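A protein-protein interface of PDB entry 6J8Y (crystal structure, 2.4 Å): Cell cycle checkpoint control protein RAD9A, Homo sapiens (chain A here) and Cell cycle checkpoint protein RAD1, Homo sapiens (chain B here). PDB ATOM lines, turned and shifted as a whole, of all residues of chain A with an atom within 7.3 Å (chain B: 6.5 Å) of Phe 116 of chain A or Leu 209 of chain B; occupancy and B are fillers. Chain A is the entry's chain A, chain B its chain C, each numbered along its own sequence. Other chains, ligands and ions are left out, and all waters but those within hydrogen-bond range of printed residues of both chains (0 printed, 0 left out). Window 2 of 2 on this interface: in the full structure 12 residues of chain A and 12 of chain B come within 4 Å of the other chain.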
ATOM      1  N   LYS A  92     -11.022 -24.082 -19.752  1.00  0.00           N
ATOM      2  CA  LYS A  92     -11.982 -24.937 -19.063  1.00  0.00           C
ATOM      3  C   LYS A  92     -12.412 -24.396 -17.701  1.00  0.00           C
ATOM      4  O   LYS A  92     -13.586 -24.480 -17.347  1.00  0.00           O
ATOM      5  CB  LYS A  92     -11.413 -26.348 -18.894  1.00  0.00           C
ATOM      6  CG  LYS A  92     -12.400 -27.328 -18.272  1.00  0.00           C
ATOM      7  CD  LYS A  92     -11.736 -28.629 -17.850  1.00  0.00           C
ATOM      8  CE  LYS A  92     -12.779 -29.670 -17.464  1.00  0.00           C
ATOM      9  NZ  LYS A  92     -13.910 -29.724 -18.436  1.00  0.00           N
ATOM     10  N   THR A  93     -11.475 -23.842 -16.936  1.00  0.00           N
ATOM     11  CA  THR A  93     -11.783 -23.446 -15.564  1.00  0.00           C
ATOM     12  C   THR A  93     -11.770 -21.934 -15.327  1.00  0.00           C
ATOM     13  O   THR A  93     -12.521 -21.434 -14.492  1.00  0.00           O
ATOM     14  CB  THR A  93     -10.805 -24.100 -14.562  1.00  0.00           C
ATOM     15  OG1 THR A  93      -9.573 -23.369 -14.535  1.00  0.00           O
ATOM     16  CG2 THR A  93     -10.535 -25.551 -14.938  1.00  0.00           C
ATOM     17  N   GLU A  95     -12.620 -18.171 -15.755  1.00  0.00           N
ATOM     18  CA  GLU A  95     -13.713 -17.367 -16.292  1.00  0.00           C
ATOM     19  C   GLU A  95     -13.314 -15.900 -16.435  1.00  0.00           C
ATOM     20  O   GLU A  95     -13.717 -15.228 -17.384  1.00  0.00           O
ATOM     21  CB  GLU A  95     -14.950 -17.496 -15.401  1.00  0.00           C
ATOM     22  CG  GLU A  95     -15.525 -18.904 -15.350  1.00  0.00           C
ATOM     23  CD  GLU A  95     -16.697 -19.028 -14.394  1.00  0.00           C
ATOM     24  OE1 GLU A  95     -16.834 -18.167 -13.501  1.00  0.00           O
ATOM     25  OE2 GLU A  95     -17.482 -19.991 -14.538  1.00  0.00           O
ATOM     26  N   CYS A 114     -11.984 -18.586 -11.131  1.00  0.00           N
ATOM     27  CA  CYS A 114     -12.252 -19.881 -11.743  1.00  0.00           C
ATOM     28  C   CYS A 114     -13.608 -20.451 -11.340  1.00  0.00           C
ATOM     29  O   CYS A 114     -14.302 -19.891 -10.490  1.00  0.00           O
ATOM     30  CB  CYS A 114     -11.144 -20.870 -11.376  1.00  0.00           C
ATOM     31  SG  CYS A 114      -9.473 -20.268 -11.732  1.00  0.00           S
ATOM     32  N   LYS A 115     -13.973 -21.568 -11.962  1.00  0.00           N
ATOM     33  CA  LYS A 115     -15.250 -22.224 -11.701  1.00  0.00           C
ATOM     34  C   LYS A 115     -15.374 -22.690 -10.255  1.00  0.00           C
ATOM     35  O   LYS A 115     -14.371 -22.888  -9.568  1.00  0.00           O
ATOM     36  CB  LYS A 115     -15.438 -23.415 -12.644  1.00  0.00           C
ATOM     37  CG  LYS A 115     -15.780 -23.035 -14.073  1.00  0.00           C
ATOM     38  CD  LYS A 115     -15.952 -24.271 -14.941  1.00  0.00           C
ATOM     39  CE  LYS A 115     -16.502 -23.913 -16.311  1.00  0.00           C
ATOM     40  NZ  LYS A 115     -16.549 -25.099 -17.212  1.00  0.00           N
ATOM     41  N   PHE A 116     -16.618 -22.854  -9.809  1.00  0.00           N
ATOM     42  CA  PHE A 116     -16.936 -23.310  -8.457  1.00  0.00           C
ATOM     43  C   PHE A 116     -16.369 -22.384  -7.383  1.00  0.00           C
ATOM     44  O   PHE A 116     -16.074 -22.819  -6.271  1.00  0.00           O
ATOM     45  CB  PHE A 116     -16.428 -24.738  -8.237  1.00  0.00           C
ATOM     46  CG  PHE A 116     -16.679 -25.656  -9.400  1.00  0.00           C
ATOM     47  CD1 PHE A 116     -17.971 -25.936  -9.813  1.00  0.00           C
ATOM     48  CD2 PHE A 116     -15.622 -26.242 -10.076  1.00  0.00           C
ATOM     49  CE1 PHE A 116     -18.205 -26.781 -10.884  1.00  0.00           C
ATOM     50  CE2 PHE A 116     -15.847 -27.088 -11.145  1.00  0.00           C
ATOM     51  CZ  PHE A 116     -17.140 -27.358 -11.549  1.00  0.00           C
ATOM     52  N   GLY A 117     -16.218 -21.108  -7.722  1.00  0.00           N
ATOM     53  CA  GLY A 117     -15.770 -20.109  -6.768  1.00  0.00           C
ATOM     54  C   GLY A 117     -14.289 -20.165  -6.441  1.00  0.00           C
ATOM     55  O   GLY A 117     -13.816 -19.450  -5.557  1.00  0.00           O
ATOM     56  N   VAL A 118     -13.552 -21.012  -7.152  1.00  0.00           N
ATOM     57  CA  VAL A 118     -12.113 -21.130  -6.939  1.00  0.00           C
ATOM     58  C   VAL A 118     -11.391 -19.881  -7.441  1.00  0.00           C
ATOM     59  O   VAL A 118     -11.686 -19.377  -8.524  1.00  0.00           O
ATOM     60  CB  VAL A 118     -11.539 -22.374  -7.639  1.00  0.00           C
ATOM     61  CG1 VAL A 118     -10.053 -22.516  -7.348  1.00  0.00           C
ATOM     62  CG2 VAL A 118     -12.289 -23.616  -7.195  1.00  0.00           C
ATOM     63  N   ARG A 119     -10.450 -19.384  -6.644  1.00  0.00           N
ATOM     64  CA  ARG A 119      -9.710 -18.180  -6.998  1.00  0.00           C
ATOM     65  C   ARG A 119      -8.206 -18.391  -6.841  1.00  0.00           C
ATOM     66  O   ARG A 119      -7.731 -18.753  -5.765  1.00  0.00           O
ATOM     67  CB  ARG A 119     -10.177 -17.003  -6.140  1.00  0.00           C
ATOM     68  CG  ARG A 119      -9.477 -15.688  -6.434  1.00  0.00           C
ATOM     69  CD  ARG A 119     -10.226 -14.525  -5.805  1.00  0.00           C
ATOM     70  NE  ARG A 119      -9.525 -13.973  -4.650  1.00  0.00           N
ATOM     71  CZ  ARG A 119     -10.049 -13.081  -3.818  1.00  0.00           C
ATOM     72  NH1 ARG A 119     -11.286 -12.640  -4.008  1.00  0.00           N
ATOM     73  NH2 ARG A 119      -9.340 -12.630  -2.792  1.00  0.00           N
ATOM     74  N   ILE B 157     -13.537 -32.536   2.902  1.00  0.00           N
ATOM     75  CA  ILE B 157     -13.680 -33.519   1.837  1.00  0.00           C
ATOM     76  C   ILE B 157     -13.973 -32.814   0.522  1.00  0.00           C
ATOM     77  O   ILE B 157     -14.922 -32.038   0.418  1.00  0.00           O
ATOM     78  CB  ILE B 157     -14.794 -34.532   2.133  1.00  0.00           C
ATOM     79  CG1 ILE B 157     -14.472 -35.313   3.407  1.00  0.00           C
ATOM     80  CG2 ILE B 157     -14.972 -35.483   0.960  1.00  0.00           C
ATOM     81  CD1 ILE B 157     -15.544 -36.302   3.795  1.00  0.00           C
ATOM     82  N   LEU B 158     -13.153 -33.093  -0.482  1.00  0.00           N
ATOM     83  CA  LEU B 158     -13.257 -32.405  -1.756  1.00  0.00           C
ATOM     84  C   LEU B 158     -13.419 -33.362  -2.933  1.00  0.00           C
ATOM     85  O   LEU B 158     -12.906 -34.480  -2.915  1.00  0.00           O
ATOM     86  CB  LEU B 158     -12.024 -31.533  -1.970  1.00  0.00           C
ATOM     87  CG  LEU B 158     -11.884 -30.205  -1.226  1.00  0.00           C
ATOM     88  CD1 LEU B 158     -10.419 -29.902  -0.956  1.00  0.00           C
ATOM     89  CD2 LEU B 158     -12.516 -29.086  -2.033  1.00  0.00           C
ATOM     90  N   GLN B 159     -14.146 -32.912  -3.952  1.00  0.00           N
ATOM     91  CA  GLN B 159     -14.229 -33.639  -5.211  1.00  0.00           C
ATOM     92  C   GLN B 159     -12.883 -33.557  -5.913  1.00  0.00           C
ATOM     93  O   GLN B 159     -12.436 -32.473  -6.268  1.00  0.00           O
ATOM     94  CB  GLN B 159     -15.331 -33.066  -6.102  1.00  0.00           C
ATOM     95  CG  GLN B 159     -16.661 -33.784  -5.989  1.00  0.00           C
ATOM     96  CD  GLN B 159     -17.812 -32.953  -6.516  1.00  0.00           C
ATOM     97  OE1 GLN B 159     -17.633 -32.108  -7.394  1.00  0.00           O
ATOM     98  NE2 GLN B 159     -19.005 -33.189  -5.983  1.00  0.00           N
ATOM     99  N   SER B 160     -12.244 -34.704  -6.115  1.00  0.00           N
ATOM    100  CA  SER B 160     -10.877 -34.736  -6.627  1.00  0.00           C
ATOM    101  C   SER B 160     -10.705 -34.137  -8.025  1.00  0.00           C
ATOM    102  O   SER B 160      -9.735 -33.418  -8.258  1.00  0.00           O
ATOM    103  CB  SER B 160     -10.348 -36.172  -6.631  1.00  0.00           C
ATOM    104  OG  SER B 160     -10.085 -36.630  -5.316  1.00  0.00           O
ATOM    105  N   GLU B 161     -11.626 -34.430  -8.945  1.00  0.00           N
ATOM    106  CA  GLU B 161     -11.437 -34.070 -10.356  1.00  0.00           C
ATOM    107  C   GLU B 161     -11.210 -32.579 -10.495  1.00  0.00           C
ATOM    108  O   GLU B 161     -10.206 -32.172 -11.068  1.00  0.00           O
ATOM    109  CB  GLU B 161     -12.630 -34.515 -11.218  1.00  0.00           C
ATOM    110  CG  GLU B 161     -12.279 -34.909 -12.685  1.00  0.00           C
ATOM    111  CD  GLU B 161     -11.674 -33.788 -13.538  1.00  0.00           C
ATOM    112  OE1 GLU B 161     -12.026 -32.608 -13.329  1.00  0.00           O
ATOM    113  OE2 GLU B 161     -10.821 -34.090 -14.402  1.00  0.00           O
ATOM    114  N   GLY B 162     -12.107 -31.777  -9.925  1.00  0.00           N
ATOM    115  CA  GLY B 162     -12.014 -30.329  -9.994  1.00  0.00           C
ATOM    116  C   GLY B 162     -10.804 -29.744  -9.305  1.00  0.00           C
ATOM    117  O   GLY B 162     -10.702 -28.535  -9.139  1.00  0.00           O
ATOM    118  N   LEU B 163      -9.868 -30.587  -8.899  1.00  0.00           N
ATOM    119  CA  LEU B 163      -8.722 -30.090  -8.139  1.00  0.00           C
ATOM    120  C   LEU B 163      -7.381 -30.509  -8.747  1.00  0.00           C
ATOM    121  O   LEU B 163      -6.370 -29.857  -8.517  1.00  0.00           O
ATOM    122  CB  LEU B 163      -8.809 -30.557  -6.691  1.00  0.00           C
ATOM    123  CG  LEU B 163     -10.148 -30.505  -5.943  1.00  0.00           C
ATOM    124  CD1 LEU B 163      -9.993 -30.976  -4.519  1.00  0.00           C
ATOM    125  CD2 LEU B 163     -10.740 -29.109  -5.982  1.00  0.00           C
ATOM    126  N   TYR B 203     -10.215 -22.009  -1.931  1.00  0.00           N
ATOM    127  CA  TYR B 203     -11.471 -22.728  -2.103  1.00  0.00           C
ATOM    128  C   TYR B 203     -12.472 -22.305  -1.033  1.00  0.00           C
ATOM    129  O   TYR B 203     -12.235 -22.512   0.157  1.00  0.00           O
ATOM    130  CB  TYR B 203     -11.247 -24.241  -2.033  1.00  0.00           C
ATOM    131  CG  TYR B 203     -10.401 -24.803  -3.153  1.00  0.00           C
ATOM    132  CD1 TYR B 203      -9.016 -24.824  -3.060  1.00  0.00           C
ATOM    133  CD2 TYR B 203     -10.989 -25.321  -4.297  1.00  0.00           C
ATOM    134  CE1 TYR B 203      -8.239 -25.340  -4.082  1.00  0.00           C
ATOM    135  CE2 TYR B 203     -10.223 -25.835  -5.322  1.00  0.00           C
ATOM    136  CZ  TYR B 203      -8.850 -25.846  -5.209  1.00  0.00           C
ATOM    137  OH  TYR B 203      -8.086 -26.363  -6.232  1.00  0.00           O
ATOM    138  N   PRO B 204     -13.596 -21.705  -1.451  1.00  0.00           N
ATOM    139  CA  PRO B 204     -14.638 -21.320  -0.495  1.00  0.00           C
ATOM    140  C   PRO B 204     -15.446 -22.531  -0.038  1.00  0.00           C
ATOM    141  O   PRO B 204     -15.654 -23.448  -0.829  1.00  0.00           O
ATOM    142  CB  PRO B 204     -15.504 -20.347  -1.297  1.00  0.00           C
ATOM    143  CG  PRO B 204     -15.352 -20.803  -2.708  1.00  0.00           C
ATOM    144  CD  PRO B 204     -13.944 -21.330  -2.833  1.00  0.00           C
ATOM    145  N   ASP B 206     -18.413 -22.700   0.381  1.00  0.00           N
ATOM    146  CA  ASP B 206     -19.637 -22.641  -0.410  1.00  0.00           C
ATOM    147  C   ASP B 206     -19.540 -23.550  -1.641  1.00  0.00           C
ATOM    148  O   ASP B 206     -20.545 -24.076  -2.118  1.00  0.00           O
ATOM    149  CB  ASP B 206     -19.895 -21.185  -0.826  1.00  0.00           C
ATOM    150  CG  ASP B 206     -21.229 -20.984  -1.532  1.00  0.00           C
ATOM    151  OD1 ASP B 206     -22.027 -21.937  -1.638  1.00  0.00           O
ATOM    152  OD2 ASP B 206     -21.478 -19.847  -1.987  1.00  0.00           O
ATOM    153  N   SER B 207     -18.317 -23.745  -2.129  1.00  0.00           N
ATOM    154  CA  SER B 207     -18.062 -24.392  -3.419  1.00  0.00           C
ATOM    155  C   SER B 207     -18.740 -25.748  -3.621  1.00  0.00           C
ATOM    156  O   SER B 207     -18.987 -26.487  -2.668  1.00  0.00           O
ATOM    157  CB  SER B 207     -16.555 -24.565  -3.621  1.00  0.00           C
ATOM    158  OG  SER B 207     -16.277 -25.160  -4.875  1.00  0.00           O
ATOM    159  N   ASP B 208     -19.023 -26.061  -4.884  1.00  0.00           N
ATOM    160  CA  ASP B 208     -19.588 -27.351  -5.269  1.00  0.00           C
ATOM    161  C   ASP B 208     -18.532 -28.449  -5.227  1.00  0.00           C
ATOM    162  O   ASP B 208     -18.834 -29.624  -5.439  1.00  0.00           O
ATOM    163  CB  ASP B 208     -20.200 -27.272  -6.670  1.00  0.00           C
ATOM    164  CG  ASP B 208     -21.601 -26.695  -6.666  1.00  0.00           C
ATOM    165  OD1 ASP B 208     -21.976 -26.047  -5.666  1.00  0.00           O
ATOM    166  OD2 ASP B 208     -22.323 -26.886  -7.665  1.00  0.00           O
ATOM    167  N   LEU B 209     -17.290 -28.056  -4.970  1.00  0.00           N
ATOM    168  CA  LEU B 209     -16.198 -29.006  -4.817  1.00  0.00           C
ATOM    169  C   LEU B 209     -16.104 -29.438  -3.359  1.00  0.00           C
ATOM    170  O   LEU B 209     -15.546 -30.488  -3.044  1.00  0.00           O
ATOM    171  CB  LEU B 209     -14.879 -28.392  -5.288  1.00  0.00           C
ATOM    172  CG  LEU B 209     -14.871 -27.878  -6.729  1.00  0.00           C
ATOM    173  CD1 LEU B 209     -13.649 -27.016  -6.986  1.00  0.00           C
ATOM    174  CD2 LEU B 209     -14.927 -29.037  -7.713  1.00  0.00           C
ATOM    175  N   MET B 210     -16.656 -28.610  -2.477  1.00  0.00           N
ATOM    176  CA  MET B 210     -16.730 -28.924  -1.055  1.00  0.00           C
ATOM    177  C   MET B 210     -17.870 -29.891  -0.775  1.00  0.00           C
ATOM    178  O   MET B 210     -19.040 -29.509  -0.812  1.00  0.00           O
ATOM    179  CB  MET B 210     -16.920 -27.651  -0.228  1.00  0.00           C
ATOM    180  CG  MET B 210     -15.675 -26.801  -0.082  1.00  0.00           C
ATOM    181  SD  MET B 210     -14.429 -27.606   0.936  1.00  0.00           S
ATOM    182  CE  MET B 210     -13.206 -26.303   1.069  1.00  0.00           C
ATOM    183  N   GLU B 211     -17.531 -31.144  -0.495  1.00  0.00           N
ATOM    184  CA  GLU B 211     -18.540 -32.137  -0.156  1.00  0.00           C
ATOM    185  C   GLU B 211     -18.749 -32.169   1.352  1.00  0.00           C
ATOM    186  O   GLU B 211     -19.778 -32.635   1.840  1.00  0.00           O
ATOM    187  CB  GLU B 211     -18.138 -33.515  -0.675  1.00  0.00           C
ATOM    188  CG  GLU B 211     -19.138 -34.109  -1.647  1.00  0.00           C
ATOM    189  CD  GLU B 211     -18.539 -35.212  -2.487  1.00  0.00           C
ATOM    190  OE1 GLU B 211     -17.713 -35.976  -1.950  1.00  0.00           O
ATOM    191  OE2 GLU B 211     -18.890 -35.312  -3.682  1.00  0.00           O
ATOM    192  N   ALA B 212     -17.762 -31.656   2.079  1.00  0.00           N
ATOM    193  CA  ALA B 212     -17.832 -31.560   3.530  1.00  0.00           C
ATOM    194  C   ALA B 212     -16.829 -30.530   4.034  1.00  0.00           C
ATOM    195  O   ALA B 212     -15.659 -30.552   3.653  1.00  0.00           O
ATOM    196  CB  ALA B 212     -17.575 -32.917   4.172  1.00  0.00           C
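O of Phe 116 of chain A is in hydrogen-bond range of OG of Ser 207 of chain B, 2.7 Å away.
Of the 16 printed residues of chain B, 4 touch a printed residue of chain A.
Hydrophobic or aromatic side chains of chain A that line the printed part of chain B: Phe 116 and Val 118.
Among the printed residues, no Asp or Glu carboxylate lies within 4 Å of a Lys or Arg side-chain nitrogen of the other chain.
Among the printed residues, merely in contact across the chains: Gly 117 of chain A with Pro 204 of chain B (3.3 Å), Val 118 of chain A with Tyr 203 of chain B (3.6 Å), Val 118 of chain A with Leu 209 of chain B (3.7 Å) and Phe 116 of chain A with Leu 209 of chain B (3.7 Å).
Of the printed residues of chain B, Phe 116 of chain A touches Ser 207 and Leu 209.
Leu 209 of chain B touches just these residues of chain A: Phe 116 (3.7 Å) and Val 118 (3.7 Å).
Printed residues of chain B within 4 Å of Val 118 of chain A: Tyr 203 (3.6 Å) and Leu 209 (3.7 Å).
Of the printed residues of chain A, Pro 204 of chain B touches Gly 117.
Glu 95 of chain A touches none of the printed residues of chain B.
Arg 119 of chain A touches none of the printed residues of chain B.
The nearest residue of chain B that does not touch Phe 116 of chain A is Asp 208 of chain B (4.1 Å).
The nearest residue of chain A that does not touch Leu 209 of chain B is Lys 115 of chain A (4.9 Å).
The nearest printed residue of chain A that does not touch Tyr 203 of chain B is Gly 117 of chain A (5.3 Å).
O of Leu 209 of chain B sits at hydrogen-bond distance from N of Gln 159 of chain B, 2.9 Å away.
OG of Ser 207 of chain B sits close to N of Leu 209 of chain B (3.1 Å).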
